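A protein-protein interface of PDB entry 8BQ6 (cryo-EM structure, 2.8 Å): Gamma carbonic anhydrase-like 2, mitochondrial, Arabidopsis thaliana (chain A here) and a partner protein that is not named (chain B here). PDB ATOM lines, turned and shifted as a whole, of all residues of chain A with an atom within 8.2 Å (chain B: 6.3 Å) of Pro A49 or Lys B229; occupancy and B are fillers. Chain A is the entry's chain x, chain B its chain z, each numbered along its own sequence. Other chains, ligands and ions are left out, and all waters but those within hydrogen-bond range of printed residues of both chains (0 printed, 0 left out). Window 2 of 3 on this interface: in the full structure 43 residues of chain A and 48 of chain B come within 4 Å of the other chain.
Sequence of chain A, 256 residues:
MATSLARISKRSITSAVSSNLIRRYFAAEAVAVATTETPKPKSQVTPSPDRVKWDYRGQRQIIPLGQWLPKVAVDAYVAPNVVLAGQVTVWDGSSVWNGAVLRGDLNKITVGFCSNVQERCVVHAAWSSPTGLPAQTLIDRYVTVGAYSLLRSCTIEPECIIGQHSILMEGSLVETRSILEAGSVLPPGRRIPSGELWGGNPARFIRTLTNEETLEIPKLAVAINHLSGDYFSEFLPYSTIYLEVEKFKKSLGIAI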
ATOM      1  N   THR A  46      -8.795   1.053  -2.697  1.00  0.00           N
ATOM      2  CA  THR A  46      -9.217   1.242  -1.316  1.00  0.00           C
ATOM      3  C   THR A  46      -8.036   1.683  -0.463  1.00  0.00           C
ATOM      4  O   THR A  46      -7.078   0.914  -0.296  1.00  0.00           O
ATOM      5  CB  THR A  46      -9.853  -0.035  -0.753  1.00  0.00           C
ATOM      6  OG1 THR A  46     -10.014   0.090   0.666  1.00  0.00           O
ATOM      7  CG2 THR A  46      -9.046  -1.290  -1.096  1.00  0.00           C
ATOM      8  N   PRO A  47      -8.052   2.896   0.081  1.00  0.00           N
ATOM      9  CA  PRO A  47      -6.885   3.413   0.798  1.00  0.00           C
ATOM     10  C   PRO A  47      -6.820   2.928   2.240  1.00  0.00           C
ATOM     11  O   PRO A  47      -7.690   2.213   2.737  1.00  0.00           O
ATOM     12  CB  PRO A  47      -7.089   4.930   0.733  1.00  0.00           C
ATOM     13  CG  PRO A  47      -8.557   5.097   0.682  1.00  0.00           C
ATOM     14  CD  PRO A  47      -9.116   3.905  -0.048  1.00  0.00           C
ATOM     15  N   SER A  48      -5.735   3.330   2.903  1.00  0.00           N
ATOM     16  CA  SER A  48      -5.483   3.049   4.304  1.00  0.00           C
ATOM     17  C   SER A  48      -5.549   4.331   5.111  1.00  0.00           C
ATOM     18  O   SER A  48      -4.876   5.310   4.762  1.00  0.00           O
ATOM     19  CB  SER A  48      -4.112   2.395   4.490  1.00  0.00           C
ATOM     20  OG  SER A  48      -3.062   3.327   4.360  1.00  0.00           O
ATOM     21  N   PRO A  49      -6.360   4.375   6.171  1.00  0.00           N
ATOM     22  CA  PRO A  49      -6.327   5.538   7.069  1.00  0.00           C
ATOM     23  C   PRO A  49      -5.052   5.647   7.888  1.00  0.00           C
ATOM     24  O   PRO A  49      -4.803   6.714   8.459  1.00  0.00           O
ATOM     25  CB  PRO A  49      -7.553   5.329   7.972  1.00  0.00           C
ATOM     26  CG  PRO A  49      -8.395   4.291   7.278  1.00  0.00           C
ATOM     27  CD  PRO A  49      -7.438   3.434   6.514  1.00  0.00           C
ATOM     28  N   ASP A  50      -4.241   4.594   7.977  1.00  0.00           N
ATOM     29  CA  ASP A  50      -2.999   4.673   8.736  1.00  0.00           C
ATOM     30  C   ASP A  50      -1.775   4.960   7.873  1.00  0.00           C
ATOM     31  O   ASP A  50      -0.656   4.934   8.394  1.00  0.00           O
ATOM     32  CB  ASP A  50      -2.767   3.387   9.544  1.00  0.00           C
ATOM     33  CG  ASP A  50      -2.665   2.143   8.674  1.00  0.00           C
ATOM     34  OD1 ASP A  50      -2.689   2.256   7.432  1.00  0.00           O
ATOM     35  OD2 ASP A  50      -2.536   1.039   9.246  1.00  0.00           O
ATOM     36  N   ARG A  51      -1.946   5.218   6.578  1.00  0.00           N
ATOM     37  CA  ARG A  51      -0.796   5.526   5.738  1.00  0.00           C
ATOM     38  C   ARG A  51      -0.136   6.817   6.199  1.00  0.00           C
ATOM     39  O   ARG A  51      -0.803   7.829   6.428  1.00  0.00           O
ATOM     40  CB  ARG A  51      -1.206   5.656   4.274  1.00  0.00           C
ATOM     41  CG  ARG A  51      -0.114   6.220   3.389  1.00  0.00           C
ATOM     42  CD  ARG A  51      -0.430   6.060   1.913  1.00  0.00           C
ATOM     43  NE  ARG A  51      -0.670   4.680   1.507  1.00  0.00           N
ATOM     44  CZ  ARG A  51       0.273   3.836   1.113  1.00  0.00           C
ATOM     45  NH1 ARG A  51       1.550   4.181   1.102  1.00  0.00           N
ATOM     46  NH2 ARG A  51      -0.074   2.618   0.709  1.00  0.00           N
ATOM     47  N   VAL A  52       1.190   6.781   6.318  1.00  0.00           N
ATOM     48  CA  VAL A  52       1.944   7.930   6.804  1.00  0.00           C
ATOM     49  C   VAL A  52       2.163   8.910   5.658  1.00  0.00           C
ATOM     50  O   VAL A  52       2.814   8.586   4.658  1.00  0.00           O
ATOM     51  CB  VAL A  52       3.278   7.485   7.413  1.00  0.00           C
ATOM     52  CG1 VAL A  52       4.176   8.680   7.653  1.00  0.00           C
ATOM     53  CG2 VAL A  52       3.040   6.722   8.704  1.00  0.00           C
ATOM     54  N   LYS A  53       1.639  10.124   5.813  1.00  0.00           N
ATOM     55  CA  LYS A  53       1.757  11.148   4.785  1.00  0.00           C
ATOM     56  C   LYS A  53       2.945  12.069   5.020  1.00  0.00           C
ATOM     57  O   LYS A  53       3.612  12.472   4.063  1.00  0.00           O
ATOM     58  CB  LYS A  53       0.463  11.956   4.714  1.00  0.00           C
ATOM     59  CG  LYS A  53      -0.702  11.121   4.246  1.00  0.00           C
ATOM     60  CD  LYS A  53      -1.961  11.929   4.073  1.00  0.00           C
ATOM     61  CE  LYS A  53      -3.111  11.020   3.663  1.00  0.00           C
ATOM     62  NZ  LYS A  53      -3.146   9.765   4.469  1.00  0.00           N
ATOM     63  N   TRP A  54       3.220  12.417   6.274  1.00  0.00           N
ATOM     64  CA  TRP A  54       4.437  13.130   6.637  1.00  0.00           C
ATOM     65  C   TRP A  54       5.187  12.304   7.669  1.00  0.00           C
ATOM     66  O   TRP A  54       4.637  11.974   8.723  1.00  0.00           O
ATOM     67  CB  TRP A  54       4.140  14.527   7.188  1.00  0.00           C
ATOM     68  CG  TRP A  54       5.349  15.167   7.789  1.00  0.00           C
ATOM     69  CD1 TRP A  54       6.499  15.505   7.146  1.00  0.00           C
ATOM     70  CD2 TRP A  54       5.548  15.501   9.167  1.00  0.00           C
ATOM     71  NE1 TRP A  54       7.395  16.049   8.029  1.00  0.00           N
ATOM     72  CE2 TRP A  54       6.835  16.055   9.278  1.00  0.00           C
ATOM     73  CE3 TRP A  54       4.761  15.392  10.315  1.00  0.00           C
ATOM     74  CZ2 TRP A  54       7.352  16.498  10.488  1.00  0.00           C
ATOM     75  CZ3 TRP A  54       5.275  15.836  11.514  1.00  0.00           C
ATOM     76  CH2 TRP A  54       6.557  16.382  11.592  1.00  0.00           C
ATOM     77  N   TYR A  56       8.346  12.478  10.113  1.00  0.00           N
ATOM     78  CA  TYR A  56       9.281  13.437  10.695  1.00  0.00           C
ATOM     79  C   TYR A  56      10.730  12.995  10.555  1.00  0.00           C
ATOM     80  O   TYR A  56      11.625  13.844  10.556  1.00  0.00           O
ATOM     81  CB  TYR A  56       8.955  13.680  12.170  1.00  0.00           C
ATOM     82  CG  TYR A  56       9.317  12.536  13.087  1.00  0.00           C
ATOM     83  CD1 TYR A  56       8.415  11.514  13.335  1.00  0.00           C
ATOM     84  CD2 TYR A  56      10.556  12.480  13.711  1.00  0.00           C
ATOM     85  CE1 TYR A  56       8.735  10.471  14.170  1.00  0.00           C
ATOM     86  CE2 TYR A  56      10.885  11.437  14.547  1.00  0.00           C
ATOM     87  CZ  TYR A  56       9.970  10.435  14.773  1.00  0.00           C
ATOM     88  OH  TYR A  56      10.286   9.389  15.606  1.00  0.00           O
ATOM     89  N   VAL B 224       0.328  17.290  13.587  1.00  0.00           N
ATOM     90  CA  VAL B 224       0.648  16.529  14.786  1.00  0.00           C
ATOM     91  C   VAL B 224       0.122  15.106  14.724  1.00  0.00           C
ATOM     92  O   VAL B 224       0.766  14.201  15.258  1.00  0.00           O
ATOM     93  CB  VAL B 224       0.089  17.234  16.029  1.00  0.00           C
ATOM     94  CG1 VAL B 224       1.023  18.338  16.453  1.00  0.00           C
ATOM     95  CG2 VAL B 224      -1.294  17.789  15.734  1.00  0.00           C
ATOM     96  N   ILE B 225      -1.035  14.890  14.097  1.00  0.00           N
ATOM     97  CA  ILE B 225      -1.629  13.559  14.052  1.00  0.00           C
ATOM     98  C   ILE B 225      -0.702  12.577  13.348  1.00  0.00           C
ATOM     99  O   ILE B 225      -0.536  11.435  13.794  1.00  0.00           O
ATOM    100  CB  ILE B 225      -3.013  13.626  13.381  1.00  0.00           C
ATOM    101  CG1 ILE B 225      -3.952  14.504  14.207  1.00  0.00           C
ATOM    102  CG2 ILE B 225      -3.607  12.240  13.230  1.00  0.00           C
ATOM    103  CD1 ILE B 225      -3.761  14.369  15.706  1.00  0.00           C
ATOM    104  N   GLU B 226      -0.084  12.995  12.240  1.00  0.00           N
ATOM    105  CA  GLU B 226       0.889  12.125  11.589  1.00  0.00           C
ATOM    106  C   GLU B 226       2.049  11.814  12.526  1.00  0.00           C
ATOM    107  O   GLU B 226       2.528  10.673  12.575  1.00  0.00           O
ATOM    108  CB  GLU B 226       1.399  12.759  10.294  1.00  0.00           C
ATOM    109  CG  GLU B 226       0.315  13.120   9.293  1.00  0.00           C
ATOM    110  CD  GLU B 226      -0.045  11.973   8.371  1.00  0.00           C
ATOM    111  OE1 GLU B 226      -1.242  11.832   8.038  1.00  0.00           O
ATOM    112  OE2 GLU B 226       0.862  11.206   7.988  1.00  0.00           O
ATOM    113  N   PHE B 227       2.506  12.814  13.283  1.00  0.00           N
ATOM    114  CA  PHE B 227       3.595  12.603  14.231  1.00  0.00           C
ATOM    115  C   PHE B 227       3.220  11.553  15.272  1.00  0.00           C
ATOM    116  O   PHE B 227       3.986  10.618  15.531  1.00  0.00           O
ATOM    117  CB  PHE B 227       3.955  13.932  14.897  1.00  0.00           C
ATOM    118  CG  PHE B 227       5.237  13.902  15.683  1.00  0.00           C
ATOM    119  CD1 PHE B 227       6.458  13.922  15.037  1.00  0.00           C
ATOM    120  CD2 PHE B 227       5.220  13.891  17.066  1.00  0.00           C
ATOM    121  CE1 PHE B 227       7.635  13.909  15.752  1.00  0.00           C
ATOM    122  CE2 PHE B 227       6.398  13.880  17.783  1.00  0.00           C
ATOM    123  CZ  PHE B 227       7.606  13.888  17.124  1.00  0.00           C
ATOM    124  N   GLU B 228       2.031  11.683  15.866  1.00  0.00           N
ATOM    125  CA  GLU B 228       1.603  10.723  16.878  1.00  0.00           C
ATOM    126  C   GLU B 228       1.407   9.334  16.288  1.00  0.00           C
ATOM    127  O   GLU B 228       1.690   8.334  16.958  1.00  0.00           O
ATOM    128  CB  GLU B 228       0.320  11.197  17.556  1.00  0.00           C
ATOM    129  CG  GLU B 228       0.237  12.696  17.714  1.00  0.00           C
ATOM    130  CD  GLU B 228      -0.400  13.120  19.011  1.00  0.00           C
ATOM    131  OE1 GLU B 228      -0.441  12.297  19.945  1.00  0.00           O
ATOM    132  OE2 GLU B 228      -0.859  14.278  19.095  1.00  0.00           O
ATOM    133  N   LYS B 229       0.921   9.249  15.048  1.00  0.00           N
ATOM    134  CA  LYS B 229       0.778   7.949  14.400  1.00  0.00           C
ATOM    135  C   LYS B 229       2.132   7.284  14.178  1.00  0.00           C
ATOM    136  O   LYS B 229       2.283   6.079  14.411  1.00  0.00           O
ATOM    137  CB  LYS B 229       0.028   8.101  13.078  1.00  0.00           C
ATOM    138  CG  LYS B 229       0.567   7.227  11.957  1.00  0.00           C
ATOM    139  CD  LYS B 229      -0.395   7.151  10.793  1.00  0.00           C
ATOM    140  CE  LYS B 229      -0.932   8.519  10.430  1.00  0.00           C
ATOM    141  NZ  LYS B 229      -2.099   8.419   9.514  1.00  0.00           N
ATOM    142  N   VAL B 230       3.129   8.046  13.723  1.00  0.00           N
ATOM    143  CA  VAL B 230       4.458   7.466  13.544  1.00  0.00           C
ATOM    144  C   VAL B 230       5.039   7.055  14.891  1.00  0.00           C
ATOM    145  O   VAL B 230       5.709   6.021  15.008  1.00  0.00           O
ATOM    146  CB  VAL B 230       5.388   8.442  12.798  1.00  0.00           C
ATOM    147  CG1 VAL B 230       6.789   7.870  12.699  1.00  0.00           C
ATOM    148  CG2 VAL B 230       4.859   8.736  11.405  1.00  0.00           C
ATOM    149  N   LEU B 231       4.780   7.850  15.932  1.00  0.00           N
ATOM    150  CA  LEU B 231       5.349   7.570  17.247  1.00  0.00           C
ATOM    151  C   LEU B 231       4.749   6.315  17.872  1.00  0.00           C
ATOM    152  O   LEU B 231       5.470   5.505  18.465  1.00  0.00           O
ATOM    153  CB  LEU B 231       5.140   8.773  18.164  1.00  0.00           C
ATOM    154  CG  LEU B 231       6.122   9.929  17.986  1.00  0.00           C
ATOM    155  CD1 LEU B 231       6.199  10.739  19.259  1.00  0.00           C
ATOM    156  CD2 LEU B 231       7.492   9.410  17.601  1.00  0.00           C
ATOM    157  N   ARG B 232       3.433   6.136  17.755  1.00  0.00           N
ATOM    158  CA  ARG B 232       2.730   5.068  18.452  1.00  0.00           C
ATOM    159  C   ARG B 232       2.550   3.813  17.604  1.00  0.00           C
ATOM    160  O   ARG B 232       1.607   3.048  17.839  1.00  0.00           O
ATOM    161  CB  ARG B 232       1.368   5.566  18.941  1.00  0.00           C
ATOM    162  CG  ARG B 232       1.444   6.767  19.866  1.00  0.00           C
ATOM    163  CD  ARG B 232       0.071   7.366  20.105  1.00  0.00           C
ATOM    164  NE  ARG B 232       0.133   8.519  20.994  1.00  0.00           N
ATOM    165  CZ  ARG B 232      -0.885   9.331  21.244  1.00  0.00           C
ATOM    166  NH1 ARG B 232      -2.076   9.137  20.701  1.00  0.00           N
ATOM    167  NH2 ARG B 232      -0.701  10.372  22.051  1.00  0.00           N
ATOM    168  N   LYS B 233       3.428   3.578  16.634  1.00  0.00           N
ATOM    169  CA  LYS B 233       3.312   2.395  15.796  1.00  0.00           C
ATOM    170  C   LYS B 233       3.758   1.152  16.562  1.00  0.00           C
ATOM    171  O   LYS B 233       4.603   1.214  17.458  1.00  0.00           O
ATOM    172  CB  LYS B 233       4.144   2.567  14.523  1.00  0.00           C
ATOM    173  CG  LYS B 233       3.590   1.858  13.288  1.00  0.00           C
ATOM    174  CD  LYS B 233       3.957   0.383  13.251  1.00  0.00           C
ATOM    175  CE  LYS B 233       3.419  -0.307  12.004  1.00  0.00           C
ATOM    176  NZ  LYS B 233       3.994   0.242  10.744  1.00  0.00           N
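The side-chain hydroxyl (OG) of Ser A48 lies close to the side-chain carboxylate (OD1) of Asp A50 (3.3 Å). The backbone NH of Arg A51 sits close to the side-chain hydroxyl of Ser A48, 3.1 Å away. The side-chain amino group (NZ) of Lys B229 is in salt-bridge range of the side-chain carboxylate (OE1) of Glu B226 (3.8 Å).
Along chain B the printed residues that touch a printed residue of chain A span positions 226 to 231. Of the 10 printed residues of chain A, 7 touch a printed residue of chain B. Printed residues of chain A that touch a printed residue of chain B: Pro A49, Asp A50, Arg A51, Val A52, Lys A53, Trp A54 and Tyr A56. Hydrophobic or aromatic side chains of chain A within 4 Å of the printed part of chain B: Val A52 and Tyr A56. Among the printed residues, 10 pairs touch across the chains.
O of Pro A49 is in hydrogen-bond range of NZ of Lys B229 (3.4 Å). The backbone carbonyl oxygen (O) of Arg A51 sits at hydrogen-bond distance from the side-chain amino group (NZ) of Lys B229, at 3.4 Å. The side-chain carboxylate of Glu B226 lies within hydrogen-bond range of the backbone NH of Lys A53 (2.6 Å). The backbone NH of Trp A54 sits at hydrogen-bond distance from the side-chain carboxylate of Glu B226, at 3.2 Å.
Ser A48 touches none of the printed residues of chain B. Of chain B, only Lys B229 comes within 4 Å of Pro A49. Of the printed residues of chain B, Asp A50 touches Lys B229 (3.3 Å). Printed residues of chain B within 4 Å of Arg A51: Lys B229 (3.4 Å). Glu B228 touches none of the printed residues of chain A. Of chain A, only Pro A49, Asp A50 and Arg A51 come within 4 Å of Lys B229. The nearest residue of chain B that does not touch Pro A49 is Glu B226 (6.2 Å). The nearest residue of chain A that does not touch Lys B229 is Val A52 (4.04 Å). The nearest printed residue of chain A that does not touch Phe B227 is Trp A54 (4.1 Å).
Asp A50 touches Lys B229 (O to CD, 3.3 Å). C of Val A52 touches OE2 of Glu B226, at 3.5 Å. CG1 of Val A52 touches CG2 of Val B230, 3.8 Å away. Phe B227 touches Tyr A56 (CE1 to CG, 3.4 Å). Tyr A56 touches Val B230 (CE1 to CG1, 3.6 Å). Tyr A56 touches Leu B231.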
